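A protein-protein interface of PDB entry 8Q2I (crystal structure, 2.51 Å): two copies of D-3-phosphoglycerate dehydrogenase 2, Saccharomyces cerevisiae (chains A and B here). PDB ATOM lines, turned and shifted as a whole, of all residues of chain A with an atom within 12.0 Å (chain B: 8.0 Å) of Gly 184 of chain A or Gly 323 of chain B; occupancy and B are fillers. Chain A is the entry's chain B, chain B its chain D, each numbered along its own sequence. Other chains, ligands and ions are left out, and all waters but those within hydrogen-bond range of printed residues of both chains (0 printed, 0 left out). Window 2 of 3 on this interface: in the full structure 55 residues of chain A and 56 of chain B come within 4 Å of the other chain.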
ATOM      1  N   GLY A 175      35.116   8.998  -2.005  1.00  0.00           N
ATOM      2  CA  GLY A 175      33.910   8.214  -1.818  1.00  0.00           C
ATOM      3  C   GLY A 175      33.365   8.347  -0.402  1.00  0.00           C
ATOM      4  O   GLY A 175      32.158   8.488  -0.228  1.00  0.00           O
ATOM      5  N   ASP A 176      34.276   8.313   0.586  1.00  0.00           N
ATOM      6  CA  ASP A 176      33.919   8.371   1.996  1.00  0.00           C
ATOM      7  C   ASP A 176      33.354   9.748   2.338  1.00  0.00           C
ATOM      8  O   ASP A 176      32.388   9.859   3.089  1.00  0.00           O
ATOM      9  CB  ASP A 176      35.128   8.061   2.885  1.00  0.00           C
ATOM     10  CG  ASP A 176      35.434   6.584   3.136  1.00  0.00           C
ATOM     11  OD1 ASP A 176      34.609   5.730   2.764  1.00  0.00           O
ATOM     12  OD2 ASP A 176      36.513   6.285   3.736  1.00  0.00           O
ATOM     13  N   ARG A 177      33.971  10.795   1.782  1.00  0.00           N
ATOM     14  CA  ARG A 177      33.561  12.166   2.046  1.00  0.00           C
ATOM     15  C   ARG A 177      32.121  12.373   1.586  1.00  0.00           C
ATOM     16  O   ARG A 177      31.303  12.915   2.321  1.00  0.00           O
ATOM     17  CB  ARG A 177      34.481  13.141   1.302  1.00  0.00           C
ATOM     18  CG  ARG A 177      35.925  13.165   1.784  1.00  0.00           C
ATOM     19  CD  ARG A 177      36.055  13.649   3.218  1.00  0.00           C
ATOM     20  NE  ARG A 177      35.875  12.606   4.218  1.00  0.00           N
ATOM     21  CZ  ARG A 177      36.790  11.692   4.525  1.00  0.00           C
ATOM     22  NH1 ARG A 177      38.037  11.788   4.077  1.00  0.00           N
ATOM     23  NH2 ARG A 177      36.440  10.706   5.324  1.00  0.00           N
ATOM     24  N   SER A 178      31.833  11.909   0.364  1.00  0.00           N
ATOM     25  CA  SER A 178      30.534  12.117  -0.260  1.00  0.00           C
ATOM     26  C   SER A 178      29.448  11.321   0.473  1.00  0.00           C
ATOM     27  O   SER A 178      28.365  11.843   0.720  1.00  0.00           O
ATOM     28  CB  SER A 178      30.592  11.812  -1.733  1.00  0.00           C
ATOM     29  OG  SER A 178      29.462  12.373  -2.386  1.00  0.00           O
ATOM     30  N   ILE A 179      29.746  10.083   0.875  1.00  0.00           N
ATOM     31  CA  ILE A 179      28.778   9.240   1.576  1.00  0.00           C
ATOM     32  C   ILE A 179      28.414   9.869   2.926  1.00  0.00           C
ATOM     33  O   ILE A 179      27.258   9.842   3.330  1.00  0.00           O
ATOM     34  CB  ILE A 179      29.319   7.799   1.725  1.00  0.00           C
ATOM     35  CG1 ILE A 179      29.375   7.094   0.366  1.00  0.00           C
ATOM     36  CG2 ILE A 179      28.506   7.006   2.731  1.00  0.00           C
ATOM     37  CD1 ILE A 179      30.157   5.793   0.333  1.00  0.00           C
ATOM     38  N   GLU A 180      29.433  10.397   3.618  1.00  0.00           N
ATOM     39  CA  GLU A 180      29.267  11.141   4.852  1.00  0.00           C
ATOM     40  C   GLU A 180      28.307  12.310   4.629  1.00  0.00           C
ATOM     41  O   GLU A 180      27.327  12.461   5.361  1.00  0.00           O
ATOM     42  CB  GLU A 180      30.615  11.692   5.332  1.00  0.00           C
ATOM     43  CG  GLU A 180      31.572  10.681   5.937  1.00  0.00           C
ATOM     44  CD  GLU A 180      33.026  11.139   5.987  1.00  0.00           C
ATOM     45  OE1 GLU A 180      33.317  12.263   5.528  1.00  0.00           O
ATOM     46  OE2 GLU A 180      33.879  10.365   6.457  1.00  0.00           O
ATOM     47  N   LEU A 181      28.608  13.156   3.634  1.00  0.00           N
ATOM     48  CA  LEU A 181      27.865  14.391   3.424  1.00  0.00           C
ATOM     49  C   LEU A 181      26.427  14.073   3.030  1.00  0.00           C
ATOM     50  O   LEU A 181      25.516  14.765   3.473  1.00  0.00           O
ATOM     51  CB  LEU A 181      28.572  15.237   2.362  1.00  0.00           C
ATOM     52  CG  LEU A 181      29.636  16.188   2.909  1.00  0.00           C
ATOM     53  CD1 LEU A 181      30.233  17.040   1.817  1.00  0.00           C
ATOM     54  CD2 LEU A 181      29.059  17.078   3.980  1.00  0.00           C
ATOM     55  N   HIS A 182      26.241  13.006   2.226  1.00  0.00           N
ATOM     56  CA  HIS A 182      24.917  12.565   1.807  1.00  0.00           C
ATOM     57  C   HIS A 182      24.073  12.099   3.002  1.00  0.00           C
ATOM     58  O   HIS A 182      22.858  11.959   2.864  1.00  0.00           O
ATOM     59  CB  HIS A 182      24.999  11.467   0.739  1.00  0.00           C
ATOM     60  CG  HIS A 182      25.236  11.916  -0.674  1.00  0.00           C
ATOM     61  ND1 HIS A 182      26.446  12.335  -1.157  1.00  0.00           N
ATOM     62  CD2 HIS A 182      24.389  11.907  -1.740  1.00  0.00           C
ATOM     63  CE1 HIS A 182      26.342  12.596  -2.460  1.00  0.00           C
ATOM     64  NE2 HIS A 182      25.067  12.353  -2.843  1.00  0.00           N
ATOM     65  N   THR A 183      24.695  11.836   4.167  1.00  0.00           N
ATOM     66  CA  THR A 183      23.952  11.439   5.350  1.00  0.00           C
ATOM     67  C   THR A 183      24.088  12.495   6.443  1.00  0.00           C
ATOM     68  O   THR A 183      23.621  12.295   7.557  1.00  0.00           O
ATOM     69  CB  THR A 183      24.388  10.062   5.857  1.00  0.00           C
ATOM     70  OG1 THR A 183      23.615   9.864   7.037  1.00  0.00           O
ATOM     71  CG2 THR A 183      25.851   9.964   6.197  1.00  0.00           C
ATOM     72  N   GLY A 184      24.733  13.619   6.114  1.00  0.00           N
ATOM     73  CA  GLY A 184      24.739  14.790   6.972  1.00  0.00           C
ATOM     74  C   GLY A 184      26.015  14.949   7.797  1.00  0.00           C
ATOM     75  O   GLY A 184      26.072  15.817   8.656  1.00  0.00           O
ATOM     76  N   THR A 185      27.047  14.143   7.543  1.00  0.00           N
ATOM     77  CA  THR A 185      28.265  14.235   8.335  1.00  0.00           C
ATOM     78  C   THR A 185      29.307  15.084   7.605  1.00  0.00           C
ATOM     79  O   THR A 185      29.681  14.792   6.466  1.00  0.00           O
ATOM     80  CB  THR A 185      28.822  12.852   8.687  1.00  0.00           C
ATOM     81  OG1 THR A 185      27.841  12.211   9.498  1.00  0.00           O
ATOM     82  CG2 THR A 185      30.146  12.920   9.418  1.00  0.00           C
ATOM     83  N   TRP A 186      29.767  16.143   8.296  1.00  0.00           N
ATOM     84  CA  TRP A 186      30.797  17.016   7.766  1.00  0.00           C
ATOM     85  C   TRP A 186      32.124  16.592   8.377  1.00  0.00           C
ATOM     86  O   TRP A 186      32.302  16.720   9.584  1.00  0.00           O
ATOM     87  CB  TRP A 186      30.472  18.488   8.059  1.00  0.00           C
ATOM     88  CG  TRP A 186      31.480  19.450   7.499  1.00  0.00           C
ATOM     89  CD1 TRP A 186      32.710  19.740   8.012  1.00  0.00           C
ATOM     90  CD2 TRP A 186      31.357  20.230   6.294  1.00  0.00           C
ATOM     91  NE1 TRP A 186      33.360  20.648   7.224  1.00  0.00           N
ATOM     92  CE2 TRP A 186      32.548  20.984   6.169  1.00  0.00           C
ATOM     93  CE3 TRP A 186      30.367  20.365   5.309  1.00  0.00           C
ATOM     94  CZ2 TRP A 186      32.773  21.848   5.094  1.00  0.00           C
ATOM     95  CZ3 TRP A 186      30.604  21.193   4.238  1.00  0.00           C
ATOM     96  CH2 TRP A 186      31.788  21.932   4.141  1.00  0.00           C
ATOM     97  N   ASN A 187      33.044  16.077   7.552  1.00  0.00           N
ATOM     98  CA  ASN A 187      34.251  15.484   8.089  1.00  0.00           C
ATOM     99  C   ASN A 187      35.453  15.831   7.209  1.00  0.00           C
ATOM    100  O   ASN A 187      35.904  15.011   6.405  1.00  0.00           O
ATOM    101  CB  ASN A 187      34.049  13.983   8.302  1.00  0.00           C
ATOM    102  CG  ASN A 187      35.288  13.307   8.843  1.00  0.00           C
ATOM    103  OD1 ASN A 187      35.920  13.842   9.750  1.00  0.00           O
ATOM    104  ND2 ASN A 187      35.676  12.184   8.254  1.00  0.00           N
ATOM    105  N   LYS A 188      35.989  17.051   7.401  1.00  0.00           N
ATOM    106  CA  LYS A 188      37.134  17.530   6.643  1.00  0.00           C
ATOM    107  C   LYS A 188      38.403  16.879   7.178  1.00  0.00           C
ATOM    108  O   LYS A 188      38.689  16.988   8.361  1.00  0.00           O
ATOM    109  CB  LYS A 188      37.197  19.051   6.738  1.00  0.00           C
ATOM    110  CG  LYS A 188      38.197  19.764   5.841  1.00  0.00           C
ATOM    111  CD  LYS A 188      37.948  21.270   5.873  1.00  0.00           C
ATOM    112  CE  LYS A 188      39.095  22.084   5.315  1.00  0.00           C
ATOM    113  NZ  LYS A 188      38.609  23.399   4.824  1.00  0.00           N
ATOM    114  N   PRO B 317      29.701  24.239   8.185  1.00  0.00           N
ATOM    115  CA  PRO B 317      29.833  24.165   9.639  1.00  0.00           C
ATOM    116  C   PRO B 317      31.190  24.728  10.089  1.00  0.00           C
ATOM    117  O   PRO B 317      32.117  24.823   9.299  1.00  0.00           O
ATOM    118  CB  PRO B 317      29.650  22.666   9.960  1.00  0.00           C
ATOM    119  CG  PRO B 317      29.054  22.057   8.720  1.00  0.00           C
ATOM    120  CD  PRO B 317      29.580  22.905   7.582  1.00  0.00           C
ATOM    121  N   ASN B 320      33.952  19.877  12.369  1.00  0.00           N
ATOM    122  CA  ASN B 320      33.489  18.565  11.949  1.00  0.00           C
ATOM    123  C   ASN B 320      32.441  18.048  12.934  1.00  0.00           C
ATOM    124  O   ASN B 320      32.518  18.338  14.109  1.00  0.00           O
ATOM    125  CB  ASN B 320      34.679  17.627  11.738  1.00  0.00           C
ATOM    126  CG  ASN B 320      35.616  18.126  10.656  1.00  0.00           C
ATOM    127  OD1 ASN B 320      35.274  18.999   9.867  1.00  0.00           O
ATOM    128  ND2 ASN B 320      36.814  17.583  10.585  1.00  0.00           N
ATOM    129  N   GLY B 321      31.446  17.302  12.438  1.00  0.00           N
ATOM    130  CA  GLY B 321      30.419  16.721  13.288  1.00  0.00           C
ATOM    131  C   GLY B 321      29.395  15.947  12.463  1.00  0.00           C
ATOM    132  O   GLY B 321      29.423  16.016  11.239  1.00  0.00           O
ATOM    133  N   GLU B 322      28.468  15.262  13.150  1.00  0.00           N
ATOM    134  CA  GLU B 322      27.717  14.168  12.549  1.00  0.00           C
ATOM    135  C   GLU B 322      26.381  14.604  11.927  1.00  0.00           C
ATOM    136  O   GLU B 322      25.906  13.969  10.986  1.00  0.00           O
ATOM    137  CB  GLU B 322      27.506  13.047  13.565  1.00  0.00           C
ATOM    138  CG  GLU B 322      28.658  12.050  13.581  1.00  0.00           C
ATOM    139  CD  GLU B 322      28.338  10.746  14.274  1.00  0.00           C
ATOM    140  OE1 GLU B 322      27.340  10.100  13.918  1.00  0.00           O
ATOM    141  OE2 GLU B 322      29.093  10.386  15.173  1.00  0.00           O
ATOM    142  N   GLY B 323      25.738  15.632  12.464  1.00  0.00           N
ATOM    143  CA  GLY B 323      24.519  16.156  11.853  1.00  0.00           C
ATOM    144  C   GLY B 323      24.716  17.590  11.364  1.00  0.00           C
ATOM    145  O   GLY B 323      23.768  18.362  11.357  1.00  0.00           O
ATOM    146  N   SER B 324      25.951  17.937  10.969  1.00  0.00           N
ATOM    147  CA  SER B 324      26.357  19.309  10.686  1.00  0.00           C
ATOM    148  C   SER B 324      25.820  19.825   9.343  1.00  0.00           C
ATOM    149  O   SER B 324      25.591  21.027   9.192  1.00  0.00           O
ATOM    150  CB  SER B 324      27.865  19.458  10.722  1.00  0.00           C
ATOM    151  OG  SER B 324      28.355  19.429  12.054  1.00  0.00           O
ATOM    152  N   PHE B 325      25.696  18.931   8.353  1.00  0.00           N
ATOM    153  CA  PHE B 325      25.283  19.280   6.998  1.00  0.00           C
ATOM    154  C   PHE B 325      23.821  18.893   6.794  1.00  0.00           C
ATOM    155  O   PHE B 325      23.530  17.739   6.504  1.00  0.00           O
ATOM    156  CB  PHE B 325      26.187  18.567   5.992  1.00  0.00           C
ATOM    157  CG  PHE B 325      26.140  19.056   4.567  1.00  0.00           C
ATOM    158  CD1 PHE B 325      26.827  20.201   4.190  1.00  0.00           C
ATOM    159  CD2 PHE B 325      25.453  18.354   3.590  1.00  0.00           C
ATOM    160  CE1 PHE B 325      26.821  20.643   2.876  1.00  0.00           C
ATOM    161  CE2 PHE B 325      25.430  18.798   2.274  1.00  0.00           C
ATOM    162  CZ  PHE B 325      26.126  19.936   1.920  1.00  0.00           C
ATOM    163  N   ASN B 326      22.914  19.867   6.963  1.00  0.00           N
ATOM    164  CA  ASN B 326      21.483  19.591   6.989  1.00  0.00           C
ATOM    165  C   ASN B 326      20.692  20.848   6.616  1.00  0.00           C
ATOM    166  O   ASN B 326      21.297  21.884   6.307  1.00  0.00           O
ATOM    167  CB  ASN B 326      21.050  18.987   8.325  1.00  0.00           C
ATOM    168  CG  ASN B 326      21.286  19.891   9.523  1.00  0.00           C
ATOM    169  OD1 ASN B 326      21.753  21.026   9.408  1.00  0.00           O
ATOM    170  ND2 ASN B 326      20.953  19.386  10.698  1.00  0.00           N
ATOM    171  N   ASP B 327      19.350  20.717   6.643  1.00  0.00           N
ATOM    172  CA  ASP B 327      18.409  21.742   6.203  1.00  0.00           C
ATOM    173  C   ASP B 327      18.522  23.022   7.043  1.00  0.00           C
ATOM    174  O   ASP B 327      18.185  24.094   6.561  1.00  0.00           O
ATOM    175  CB  ASP B 327      16.969  21.218   6.184  1.00  0.00           C
ATOM    176  CG  ASP B 327      16.654  20.268   5.033  1.00  0.00           C
ATOM    177  OD1 ASP B 327      17.459  20.150   4.095  1.00  0.00           O
ATOM    178  OD2 ASP B 327      15.607  19.616   5.092  1.00  0.00           O
ATOM    179  N   GLU B 328      19.028  22.935   8.275  1.00  0.00           N
ATOM    180  CA  GLU B 328      19.191  24.117   9.105  1.00  0.00           C
ATOM    181  C   GLU B 328      20.419  24.920   8.660  1.00  0.00           C
ATOM    182  O   GLU B 328      20.500  26.109   8.920  1.00  0.00           O
ATOM    183  CB  GLU B 328      19.275  23.738  10.591  1.00  0.00           C
ATOM    184  CG  GLU B 328      18.208  22.777  11.122  1.00  0.00           C
ATOM    185  CD  GLU B 328      17.056  23.416  11.882  1.00  0.00           C
ATOM    186  OE1 GLU B 328      17.350  24.277  12.721  1.00  0.00           O
ATOM    187  OE2 GLU B 328      15.876  23.040  11.656  1.00  0.00           O
ATOM    188  N   LEU B 329      21.374  24.307   7.958  1.00  0.00           N
ATOM    189  CA  LEU B 329      22.570  25.021   7.525  1.00  0.00           C
ATOM    190  C   LEU B 329      22.375  25.627   6.130  1.00  0.00           C
ATOM    191  O   LEU B 329      22.769  26.780   5.890  1.00  0.00           O
ATOM    192  CB  LEU B 329      23.751  24.044   7.538  1.00  0.00           C
ATOM    193  CG  LEU B 329      25.109  24.640   7.182  1.00  0.00           C
ATOM    194  CD1 LEU B 329      25.625  25.537   8.292  1.00  0.00           C
ATOM    195  CD2 LEU B 329      26.103  23.538   6.882  1.00  0.00           C
ATOM    196  N   THR B 333      19.373  21.165   1.411  1.00  0.00           N
ATOM    197  CA  THR B 333      20.247  20.023   1.631  1.00  0.00           C
ATOM    198  C   THR B 333      19.496  18.715   1.336  1.00  0.00           C
ATOM    199  O   THR B 333      19.989  17.931   0.536  1.00  0.00           O
ATOM    200  CB  THR B 333      20.950  20.065   3.002  1.00  0.00           C
ATOM    201  OG1 THR B 333      21.793  21.216   3.197  1.00  0.00           O
ATOM    202  CG2 THR B 333      21.819  18.838   3.184  1.00  0.00           C
ATOM    203  N   VAL B 337      20.772  16.040  -1.725  1.00  0.00           N
ATOM    204  CA  VAL B 337      21.265  14.729  -1.324  1.00  0.00           C
ATOM    205  C   VAL B 337      20.510  13.605  -2.031  1.00  0.00           C
ATOM    206  O   VAL B 337      21.067  12.525  -2.222  1.00  0.00           O
ATOM    207  CB  VAL B 337      21.126  14.590   0.213  1.00  0.00           C
ATOM    208  CG1 VAL B 337      20.853  13.175   0.713  1.00  0.00           C
ATOM    209  CG2 VAL B 337      22.296  15.264   0.916  1.00  0.00           C
ATOM    210  N   LEU B 344      29.524  15.418  -3.291  1.00  0.00           N
ATOM    211  CA  LEU B 344      29.629  16.439  -2.266  1.00  0.00           C
ATOM    212  C   LEU B 344      30.885  16.194  -1.438  1.00  0.00           C
ATOM    213  O   LEU B 344      31.071  15.106  -0.902  1.00  0.00           O
ATOM    214  CB  LEU B 344      28.402  16.333  -1.362  1.00  0.00           C
ATOM    215  CG  LEU B 344      27.062  16.481  -2.073  1.00  0.00           C
ATOM    216  CD1 LEU B 344      25.901  16.355  -1.089  1.00  0.00           C
ATOM    217  CD2 LEU B 344      27.023  17.810  -2.826  1.00  0.00           C
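Of the printed residues of chain B, Arg 177 of chain A touches Leu 344.
Glu 180 of chain A touches none of the printed residues of chain B.
Printed residues of chain B within 4 Å of Leu 181 of chain A: Phe 325 (3.6 Å) and Leu 344 (3.4 Å).
Of chain B, only Glu 322 (3.0 Å), Gly 323 (3.5 Å), Ser 324 (3.1 Å) and Phe 325 (3.2 Å) come within 4 Å of Gly 184 of chain A.
Printed residues of chain A within 4 Å of Asn 320 of chain B: Trp 186 (3.2 Å), Asn 187 (3.9 Å) and Lys 188 (3.0 Å).
Gly 321 of chain B touches just these residues of chain A: Thr 185 (3.6 Å) and Trp 186 (3.0 Å).
Glu 322 of chain B touches just these residues of chain A: Gly 184 (3.0 Å) and Thr 185 (3.0 Å).
Gly 323 of chain B touches one residue of chain A.
Ser 324 of chain B touches two residues of chain A.
No residue of chain A comes within 4 Å of Asn 326 of chain B.
Thr 333 of chain B touches none of the printed residues of chain A.
Printed residues of chain A within 4 Å of Leu 344 of chain B: Arg 177 (3.8 Å), Ser 178 (3.1 Å), Leu 181 (3.4 Å) and His 182 (3.97 Å).
The nearest residue of chain A that does not touch Gly 323 of chain B is Thr 185 of chain A (5.0 Å).
The nearest printed residue of chain A that does not touch Val 337 of chain B is Leu 181 of chain A (4.1 Å).
Printed residues of chain B that touch a printed residue of chain A: Pro 317, Asn 320, Gly 321, Glu 322, Gly 323, Ser 324, Phe 325, Val 337 and Leu 344.
Of the 14 printed residues of chain A, 9 touch a printed residue of chain B.
Hydrophobic or aromatic side chains of chain A that line the printed part of chain B: Leu 181, His 182 and Trp 186.
Among the printed residues, no Asp or Glu carboxylate lies within 4 Å of a Lys or Arg side-chain nitrogen of the other chain.
No position is printed for both chains.
Of the 19 pairs that touch across the chains among the printed residues, none has its exchanged pair printed and touching as well.
N of Trp 186 of chain A sits at hydrogen-bond distance from O of Gly 321 of chain B (3.0 Å).
The backbone NH (N) of Leu 344 of chain B sits at hydrogen-bond distance from the side-chain hydroxyl (OG) of Ser 178 of chain A, at 3.2 Å.
The backbone carbonyl oxygen (O) of Gly 184 of chain A sits at hydrogen-bond distance from the backbone NH (N) of Ser 324 of chain B, 3.1 Å away.
O of Lys 188 of chain A lies within hydrogen-bond range of ND2 of Asn 320 of chain B.
The backbone carbonyl oxygen (O) of Gly 184 of chain A lies close to the backbone carbonyl oxygen (O) of Glu 322 of chain B, at 3.0 Å.
OG1 of Thr 185 of chain A is in hydrogen-bond range of O of Glu 322 of chain B.
N of Phe 325 of chain B lies within hydrogen-bond range of O of Gly 184 of chain A, at 3.2 Å.
Among the printed residues, merely in contact across the chains: Arg 177 of chain A with Leu 344 of chain B, Leu 181 of chain A with Phe 325 of chain B, Leu 181 of chain A with Leu 344 of chain B, His 182 of chain A with Val 337 of chain B, His 182 of chain A with Leu 344 of chain B, Gly 184 of chain A with Gly 323 of chain B, Thr 185 of chain A with Gly 321 of chain B, Trp 186 of chain A with Pro 317 of chain B, Trp 186 of chain A with Asn 320 of chain B, Trp 186 of chain A with Ser 324 of chain B, Trp 186 of chain A with Phe 325 of chain B and Asn 187 of chain A with Asn 320 of chain B.
A ring nitrogen (ND1) of His 182 of chain A sits at hydrogen-bond distance from the backbone carbonyl oxygen (O) of Ser 178 of chain A (2.7 Å).
The guanidinium group of Arg 177 of chain A lies within hydrogen-bond range of the backbone carbonyl oxygen of Asn 187 of chain A, 3.3 Å away.
The side-chain carboxylate (OE2) of Glu 180 of chain A sits at hydrogen-bond distance from the side-chain amide nitrogen (ND2) of Asn 187 of chain A (3.1 Å).
The guanidinium group (NH2) of Arg 177 of chain A lies within salt-bridge range of the side-chain carboxylate (OE2) of Glu 180 of chain A (2.8 Å).
The backbone carbonyl oxygen (O) of Gly 323 of chain B sits at hydrogen-bond distance from the side-chain amide nitrogen (ND2) of Asn 326 of chain B, 3.1 Å away.
N of Thr 185 of chain A is in hydrogen-bond range of O of Glu 180 of chain A, at 2.8 Å.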
